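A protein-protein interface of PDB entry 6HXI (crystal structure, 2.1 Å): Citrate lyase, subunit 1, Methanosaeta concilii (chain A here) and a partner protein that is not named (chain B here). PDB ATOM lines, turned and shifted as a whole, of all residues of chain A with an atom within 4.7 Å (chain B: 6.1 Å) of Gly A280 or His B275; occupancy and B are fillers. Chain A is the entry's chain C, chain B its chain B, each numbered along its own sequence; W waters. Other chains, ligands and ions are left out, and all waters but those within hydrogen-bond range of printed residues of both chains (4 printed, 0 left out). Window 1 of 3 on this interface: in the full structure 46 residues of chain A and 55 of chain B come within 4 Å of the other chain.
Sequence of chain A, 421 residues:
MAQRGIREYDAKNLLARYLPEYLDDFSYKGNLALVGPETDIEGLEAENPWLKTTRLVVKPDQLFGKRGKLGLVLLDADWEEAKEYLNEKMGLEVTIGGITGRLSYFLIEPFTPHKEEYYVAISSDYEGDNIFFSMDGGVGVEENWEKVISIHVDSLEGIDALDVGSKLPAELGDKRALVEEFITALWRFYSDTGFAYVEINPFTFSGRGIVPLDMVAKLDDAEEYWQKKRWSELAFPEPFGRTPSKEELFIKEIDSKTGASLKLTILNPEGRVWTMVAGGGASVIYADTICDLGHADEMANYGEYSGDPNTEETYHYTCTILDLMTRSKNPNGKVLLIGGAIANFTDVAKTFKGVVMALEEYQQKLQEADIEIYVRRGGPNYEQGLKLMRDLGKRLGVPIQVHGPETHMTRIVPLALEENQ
Water W1 lies within hydrogen-bond range of the side-chain hydroxyl of Ser B178 (2.7 Å), a ring nitrogen (NE2) of His B275 (2.8 Å), the backbone NH of Gly A281 (3.2 Å) and the backbone NH of Gly A280 (3.5 Å). Water W4 lies within hydrogen-bond range of N of His B275, O of Gly A280 and N of Gly B274. Water W2 lies within hydrogen-bond range of the backbone NH (N) of Gly A280 (3.2 Å) and a ring nitrogen (NE2) of His B275 (3.3 Å). Water W3 lies within hydrogen-bond range of the backbone NH of Ala A282 (3.3 Å) and the side-chain hydroxyl of Ser B178 (3.3 Å).
The side-chain hydroxyl (OH) of Tyr A302 is in hydrogen-bond range of the backbone NH (N) of Gly B274, 2.8 Å away.
The side-chain hydroxyl (OG) of Ser A283 is in hydrogen-bond range of the backbone carbonyl oxygen (O) of Gly A280 (3.0 Å). The side-chain hydroxyl (OG) of Ser A283 sits at hydrogen-bond distance from the side-chain hydroxyl (OH) of Tyr A302, 2.7 Å away. A ring nitrogen (ND1) of His B275 lies within hydrogen-bond range of the side-chain carboxylate (OE1) of Glu B233, at 2.9 Å. The side-chain amide nitrogen of Gln B272 is in hydrogen-bond range of the backbone carbonyl oxygen of His B275. The backbone carbonyl oxygen (O) of Ala B278 sits at hydrogen-bond distance from the backbone NH (N) of Phe B273, 3.0 Å away.
Of the 17 printed residues of chain B, 4 touch a printed residue of chain A. Hydrophobic or aromatic side chains of chain B that line the printed part of chain A: Phe B273 and His B275. Printed residues of chain A that touch a printed residue of chain B: Gly A280, Gly A281, Val A284, Tyr A302 and Glu A304. Hydrophobic or aromatic side chains of chain A that line the printed part of chain B: Val A284 and Tyr A302. Among the printed residues, 7 pairs touch across the chains. Among the printed residues, no Asp or Glu carboxylate lies within 4 Å of a Lys or Arg side-chain nitrogen of the other chain.
Of chain B, only His B275 comes within 4 Å of Gly A280. Printed residues of chain B within 4 Å of Gly A281: Ser B178 (3.4 Å) and His B275 (3.6 Å). Of the printed residues of chain B, Tyr A302 touches Phe B273 (3.7 Å) and Gly B274 (2.8 Å). Printed residues of chain B within 4 Å of Glu A304: Gly B274. Ala B139 touches none of the printed residues of chain A. Printed residues of chain A within 4 Å of Phe B273: Val A284 (3.9 Å) and Tyr A302 (3.7 Å). His B275 touches just these residues of chain A: Gly A280 (3.8 Å) and Gly A281 (3.6 Å). The nearest printed residue of chain A that does not touch His B275 is Glu A304 (4.9 Å). The nearest printed residue of chain B that does not touch Val A284 is Glu B233 (4.8 Å).
CA of Gly A280 touches NE2 of His B275 (3.8 Å). CA of Gly A281 touches OG of Ser B178, at 3.4 Å. Gly A281 touches His B275. Phe B273 touches Val A284 (CB to CG2, 3.9 Å). Phe B273 touches Tyr A302 (CD1 to CE1, 3.7 Å). Gly B274 touches Glu A304 (CA to OE1, 3.6 Å).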
ATOM      1  N   ALA A 278      -8.348  -1.396   3.480  1.00  0.00           N
ATOM      2  CA  ALA A 278      -7.327  -2.379   3.244  1.00  0.00           C
ATOM      3  C   ALA A 278      -7.898  -3.794   3.411  1.00  0.00           C
ATOM      4  O   ALA A 278      -8.529  -4.103   4.429  1.00  0.00           O
ATOM      5  CB  ALA A 278      -6.184  -2.157   4.200  1.00  0.00           C
ATOM      6  N   GLY A 279      -7.712  -4.627   2.397  1.00  0.00           N
ATOM      7  CA  GLY A 279      -8.128  -6.026   2.443  1.00  0.00           C
ATOM      8  C   GLY A 279      -9.445  -6.356   1.787  1.00  0.00           C
ATOM      9  O   GLY A 279     -10.394  -5.572   1.856  1.00  0.00           O
ATOM     10  N   GLY A 280      -9.492  -7.516   1.139  1.00  0.00           N
ATOM     11  CA  GLY A 280     -10.700  -8.027   0.498  1.00  0.00           C
ATOM     12  C   GLY A 280     -11.802  -8.310   1.505  1.00  0.00           C
ATOM     13  O   GLY A 280     -12.944  -7.894   1.300  1.00  0.00           O
ATOM     14  N   GLY A 281     -11.452  -8.993   2.605  1.00  0.00           N
ATOM     15  CA  GLY A 281     -12.378  -9.341   3.682  1.00  0.00           C
ATOM     16  C   GLY A 281     -12.999  -8.145   4.370  1.00  0.00           C
ATOM     17  O   GLY A 281     -14.225  -8.034   4.432  1.00  0.00           O
ATOM     18  N   ALA A 282     -12.152  -7.233   4.886  1.00  0.00           N
ATOM     19  CA  ALA A 282     -12.558  -6.023   5.605  1.00  0.00           C
ATOM     20  C   ALA A 282     -13.360  -5.015   4.775  1.00  0.00           C
ATOM     21  O   ALA A 282     -14.268  -4.392   5.327  1.00  0.00           O
ATOM     22  CB  ALA A 282     -11.341  -5.346   6.198  1.00  0.00           C
ATOM     23  N   SER A 283     -13.035  -4.844   3.464  1.00  0.00           N
ATOM     24  CA  SER A 283     -13.727  -3.873   2.598  1.00  0.00           C
ATOM     25  C   SER A 283     -15.192  -4.225   2.390  1.00  0.00           C
ATOM     26  O   SER A 283     -16.050  -3.341   2.328  1.00  0.00           O
ATOM     27  CB  SER A 283     -13.005  -3.712   1.269  1.00  0.00           C
ATOM     28  OG  SER A 283     -12.804  -4.967   0.641  1.00  0.00           O
ATOM     29  N   VAL A 284     -15.464  -5.534   2.310  1.00  0.00           N
ATOM     30  CA  VAL A 284     -16.787  -6.136   2.162  1.00  0.00           C
ATOM     31  C   VAL A 284     -17.550  -5.847   3.445  1.00  0.00           C
ATOM     32  O   VAL A 284     -18.696  -5.399   3.378  1.00  0.00           O
ATOM     33  CB  VAL A 284     -16.653  -7.659   1.855  1.00  0.00           C
ATOM     34  CG1 VAL A 284     -17.978  -8.383   1.994  1.00  0.00           C
ATOM     35  CG2 VAL A 284     -16.069  -7.894   0.461  1.00  0.00           C
ATOM     36  N   TYR A 302     -16.631   0.961  -4.197  1.00  0.00           N
ATOM     37  CA  TYR A 302     -16.150  -0.247  -3.540  1.00  0.00           C
ATOM     38  C   TYR A 302     -14.703  -0.347  -3.979  1.00  0.00           C
ATOM     39  O   TYR A 302     -14.419  -0.534  -5.161  1.00  0.00           O
ATOM     40  CB  TYR A 302     -16.923  -1.552  -3.873  1.00  0.00           C
ATOM     41  CG  TYR A 302     -16.169  -2.753  -3.347  1.00  0.00           C
ATOM     42  CD1 TYR A 302     -16.195  -3.074  -1.991  1.00  0.00           C
ATOM     43  CD2 TYR A 302     -15.278  -3.451  -4.161  1.00  0.00           C
ATOM     44  CE1 TYR A 302     -15.367  -4.064  -1.465  1.00  0.00           C
ATOM     45  CE2 TYR A 302     -14.433  -4.433  -3.639  1.00  0.00           C
ATOM     46  CZ  TYR A 302     -14.509  -4.761  -2.297  1.00  0.00           C
ATOM     47  OH  TYR A 302     -13.711  -5.761  -1.787  1.00  0.00           O
ATOM     48  N   GLU A 304     -10.440  -1.517  -2.569  1.00  0.00           N
ATOM     49  CA  GLU A 304      -9.629  -2.460  -1.811  1.00  0.00           C
ATOM     50  C   GLU A 304      -8.160  -2.341  -2.241  1.00  0.00           C
ATOM     51  O   GLU A 304      -7.860  -2.249  -3.429  1.00  0.00           O
ATOM     52  CB  GLU A 304     -10.151  -3.878  -2.143  1.00  0.00           C
ATOM     53  CG  GLU A 304      -9.601  -5.007  -1.317  1.00  0.00           C
ATOM     54  CD  GLU A 304      -8.439  -5.739  -1.956  1.00  0.00           C
ATOM     55  OE1 GLU A 304      -8.656  -6.522  -2.909  1.00  0.00           O
ATOM     56  OE2 GLU A 304      -7.299  -5.523  -1.495  1.00  0.00           O
ATOM     57  N   GLU B 114      -1.439 -14.281  -4.732  1.00  0.00           N
ATOM     58  CA  GLU B 114      -2.743 -13.834  -5.166  1.00  0.00           C
ATOM     59  C   GLU B 114      -2.655 -13.762  -6.701  1.00  0.00           C
ATOM     60  O   GLU B 114      -1.596 -13.405  -7.241  1.00  0.00           O
ATOM     61  CB  GLU B 114      -3.037 -12.446  -4.585  1.00  0.00           C
ATOM     62  CG  GLU B 114      -4.490 -12.024  -4.813  1.00  0.00           C
ATOM     63  CD  GLU B 114      -5.083 -10.932  -3.937  1.00  0.00           C
ATOM     64  OE1 GLU B 114      -6.277 -11.055  -3.575  1.00  0.00           O
ATOM     65  OE2 GLU B 114      -4.376  -9.936  -3.649  1.00  0.00           O
ATOM     66  N   ALA B 139      -3.708 -17.273  -2.285  1.00  0.00           N
ATOM     67  CA  ALA B 139      -4.197 -15.970  -1.826  1.00  0.00           C
ATOM     68  C   ALA B 139      -4.537 -15.946  -0.328  1.00  0.00           C
ATOM     69  O   ALA B 139      -5.581 -15.430   0.074  1.00  0.00           O
ATOM     70  CB  ALA B 139      -5.386 -15.508  -2.686  1.00  0.00           C
ATOM     71  N   LYS B 177     -11.898 -17.152   5.097  1.00  0.00           N
ATOM     72  CA  LYS B 177     -11.468 -17.057   3.710  1.00  0.00           C
ATOM     73  C   LYS B 177     -10.395 -15.967   3.672  1.00  0.00           C
ATOM     74  O   LYS B 177      -9.308 -16.185   3.162  1.00  0.00           O
ATOM     75  CB  LYS B 177     -12.646 -16.722   2.782  1.00  0.00           C
ATOM     76  CG  LYS B 177     -13.257 -17.960   2.159  1.00  0.00           C
ATOM     77  CD  LYS B 177     -14.703 -17.755   1.757  1.00  0.00           C
ATOM     78  CE  LYS B 177     -15.192 -18.975   1.008  1.00  0.00           C
ATOM     79  NZ  LYS B 177     -16.590 -18.838   0.503  1.00  0.00           N
ATOM     80  N   SER B 178     -10.679 -14.827   4.304  1.00  0.00           N
ATOM     81  CA  SER B 178      -9.818 -13.654   4.365  1.00  0.00           C
ATOM     82  C   SER B 178      -8.620 -13.796   5.305  1.00  0.00           C
ATOM     83  O   SER B 178      -8.759 -14.260   6.436  1.00  0.00           O
ATOM     84  CB  SER B 178     -10.651 -12.440   4.764  1.00  0.00           C
ATOM     85  OG  SER B 178      -9.874 -11.283   5.021  1.00  0.00           O
ATOM     86  N   GLY B 179      -7.470 -13.318   4.840  1.00  0.00           N
ATOM     87  CA  GLY B 179      -6.240 -13.304   5.614  1.00  0.00           C
ATOM     88  C   GLY B 179      -6.229 -12.213   6.669  1.00  0.00           C
ATOM     89  O   GLY B 179      -5.893 -12.478   7.824  1.00  0.00           O
ATOM     90  N   GLY B 203      -7.999 -18.606   1.970  1.00  0.00           N
ATOM     91  CA  GLY B 203      -7.834 -17.684   0.850  1.00  0.00           C
ATOM     92  C   GLY B 203      -9.191 -17.320   0.287  1.00  0.00           C
ATOM     93  O   GLY B 203     -10.194 -17.953   0.629  1.00  0.00           O
ATOM     94  N   GLY B 204      -9.230 -16.315  -0.573  1.00  0.00           N
ATOM     95  CA  GLY B 204     -10.476 -15.853  -1.176  1.00  0.00           C
ATOM     96  C   GLY B 204     -10.734 -16.290  -2.605  1.00  0.00           C
ATOM     97  O   GLY B 204     -11.614 -15.747  -3.276  1.00  0.00           O
ATOM     98  N   ASP B 205      -9.992 -17.279  -3.078  1.00  0.00           N
ATOM     99  CA  ASP B 205     -10.156 -17.768  -4.429  1.00  0.00           C
ATOM    100  C   ASP B 205     -11.380 -18.693  -4.542  1.00  0.00           C
ATOM    101  O   ASP B 205     -11.736 -19.369  -3.568  1.00  0.00           O
ATOM    102  CB  ASP B 205      -8.863 -18.456  -4.917  1.00  0.00           C
ATOM    103  CG  ASP B 205      -7.686 -17.521  -5.244  1.00  0.00           C
ATOM    104  OD1 ASP B 205      -7.906 -16.299  -5.387  1.00  0.00           O
ATOM    105  OD2 ASP B 205      -6.562 -18.016  -5.391  1.00  0.00           O
ATOM    106  N   GLU B 233     -17.793 -15.809   3.173  1.00  0.00           N
ATOM    107  CA  GLU B 233     -18.211 -14.683   2.319  1.00  0.00           C
ATOM    108  C   GLU B 233     -19.058 -15.174   1.143  1.00  0.00           C
ATOM    109  O   GLU B 233     -19.042 -16.365   0.819  1.00  0.00           O
ATOM    110  CB  GLU B 233     -17.013 -13.808   1.847  1.00  0.00           C
ATOM    111  CG  GLU B 233     -16.085 -14.487   0.865  1.00  0.00           C
ATOM    112  CD  GLU B 233     -14.945 -13.677   0.277  1.00  0.00           C
ATOM    113  OE1 GLU B 233     -14.782 -12.483   0.637  1.00  0.00           O
ATOM    114  OE2 GLU B 233     -14.223 -14.248  -0.578  1.00  0.00           O
ATOM    115  N   GLN B 272     -17.995  -7.206  -8.619  1.00  0.00           N
ATOM    116  CA  GLN B 272     -17.013  -8.220  -8.254  1.00  0.00           C
ATOM    117  C   GLN B 272     -16.284  -7.623  -7.053  1.00  0.00           C
ATOM    118  O   GLN B 272     -15.805  -6.483  -7.127  1.00  0.00           O
ATOM    119  CB  GLN B 272     -16.042  -8.500  -9.425  1.00  0.00           C
ATOM    120  CG  GLN B 272     -14.800  -9.329  -9.060  1.00  0.00           C
ATOM    121  CD  GLN B 272     -15.095 -10.751  -8.638  1.00  0.00           C
ATOM    122  OE1 GLN B 272     -15.717 -11.528  -9.372  1.00  0.00           O
ATOM    123  NE2 GLN B 272     -14.610 -11.132  -7.464  1.00  0.00           N
ATOM    124  N   PHE B 273     -16.247  -8.357  -5.940  1.00  0.00           N
ATOM    125  CA  PHE B 273     -15.574  -7.845  -4.748  1.00  0.00           C
ATOM    126  C   PHE B 273     -14.105  -8.255  -4.730  1.00  0.00           C
ATOM    127  O   PHE B 273     -13.669  -8.957  -5.648  1.00  0.00           O
ATOM    128  CB  PHE B 273     -16.339  -8.203  -3.462  1.00  0.00           C
ATOM    129  CG  PHE B 273     -17.722  -7.596  -3.453  1.00  0.00           C
ATOM    130  CD1 PHE B 273     -17.910  -6.258  -3.128  1.00  0.00           C
ATOM    131  CD2 PHE B 273     -18.833  -8.353  -3.806  1.00  0.00           C
ATOM    132  CE1 PHE B 273     -19.193  -5.697  -3.113  1.00  0.00           C
ATOM    133  CE2 PHE B 273     -20.115  -7.793  -3.797  1.00  0.00           C
ATOM    134  CZ  PHE B 273     -20.286  -6.469  -3.450  1.00  0.00           C
ATOM    135  N   GLY B 274     -13.361  -7.737  -3.743  1.00  0.00           N
ATOM    136  CA  GLY B 274     -11.923  -7.911  -3.552  1.00  0.00           C
ATOM    137  C   GLY B 274     -11.352  -9.264  -3.894  1.00  0.00           C
ATOM    138  O   GLY B 274     -10.573  -9.381  -4.836  1.00  0.00           O
ATOM    139  N   HIS B 275     -11.754 -10.298  -3.153  1.00  0.00           N
ATOM    140  CA  HIS B 275     -11.309 -11.678  -3.395  1.00  0.00           C
ATOM    141  C   HIS B 275     -11.833 -12.185  -4.726  1.00  0.00           C
ATOM    142  O   HIS B 275     -12.975 -11.879  -5.087  1.00  0.00           O
ATOM    143  CB  HIS B 275     -11.788 -12.604  -2.269  1.00  0.00           C
ATOM    144  CG  HIS B 275     -11.205 -12.305  -0.920  1.00  0.00           C
ATOM    145  ND1 HIS B 275     -11.884 -12.617   0.236  1.00  0.00           N
ATOM    146  CD2 HIS B 275     -10.014 -11.753  -0.590  1.00  0.00           C
ATOM    147  CE1 HIS B 275     -11.099 -12.248   1.227  1.00  0.00           C
ATOM    148  NE2 HIS B 275      -9.962 -11.721   0.779  1.00  0.00           N
ATOM    149  N   ALA B 276     -11.010 -12.964  -5.457  1.00  0.00           N
ATOM    150  CA  ALA B 276     -11.414 -13.535  -6.760  1.00  0.00           C
ATOM    151  C   ALA B 276     -12.762 -14.291  -6.704  1.00  0.00           C
ATOM    152  O   ALA B 276     -13.577 -14.141  -7.613  1.00  0.00           O
ATOM    153  CB  ALA B 276     -10.315 -14.434  -7.316  1.00  0.00           C
ATOM    154  N   GLY B 277     -13.011 -15.015  -5.611  1.00  0.00           N
ATOM    155  CA  GLY B 277     -14.246 -15.775  -5.450  1.00  0.00           C
ATOM    156  C   GLY B 277     -15.430 -15.036  -4.859  1.00  0.00           C
ATOM    157  O   GLY B 277     -16.509 -15.623  -4.750  1.00  0.00           O
ATOM    158  N   ALA B 278     -15.247 -13.763  -4.440  1.00  0.00           N
ATOM    159  CA  ALA B 278     -16.319 -12.972  -3.808  1.00  0.00           C
ATOM    160  C   ALA B 278     -17.262 -12.294  -4.809  1.00  0.00           C
ATOM    161  O   ALA B 278     -17.236 -11.070  -4.965  1.00  0.00           O
ATOM    162  CB  ALA B 278     -15.742 -11.961  -2.814  1.00  0.00           C
ATOM    163  N   LYS B 279     -18.080 -13.120  -5.506  1.00  0.00           N
ATOM    164  CA  LYS B 279     -19.129 -12.702  -6.444  1.00  0.00           C
ATOM    165  C   LYS B 279     -20.278 -13.734  -6.480  1.00  0.00           C
ATOM    166  O   LYS B 279     -20.108 -14.818  -7.053  1.00  0.00           O
ATOM    167  CB  LYS B 279     -18.595 -12.410  -7.863  1.00  0.00           C
ATOM    168  CG  LYS B 279     -19.622 -11.644  -8.700  1.00  0.00           C
ATOM    169  CD  LYS B 279     -19.230 -11.470 -10.155  1.00  0.00           C
ATOM    170  CE  LYS B 279     -20.106 -10.422 -10.808  1.00  0.00           C
ATOM    171  NZ  LYS B 279     -20.352 -10.695 -12.248  1.00  0.00           N
HETATM  172  O   HOH W   1      -8.538 -10.399   2.843  1.00  0.00           O
HETATM  173  O   HOH W   2      -7.440  -9.681   0.012  1.00  0.00           O
HETATM  174  O   HOH W   3      -9.055  -8.090   5.409  1.00  0.00           O
HETATM  175  O   HOH W   4     -13.631  -9.684  -1.201  1.00  0.00           O
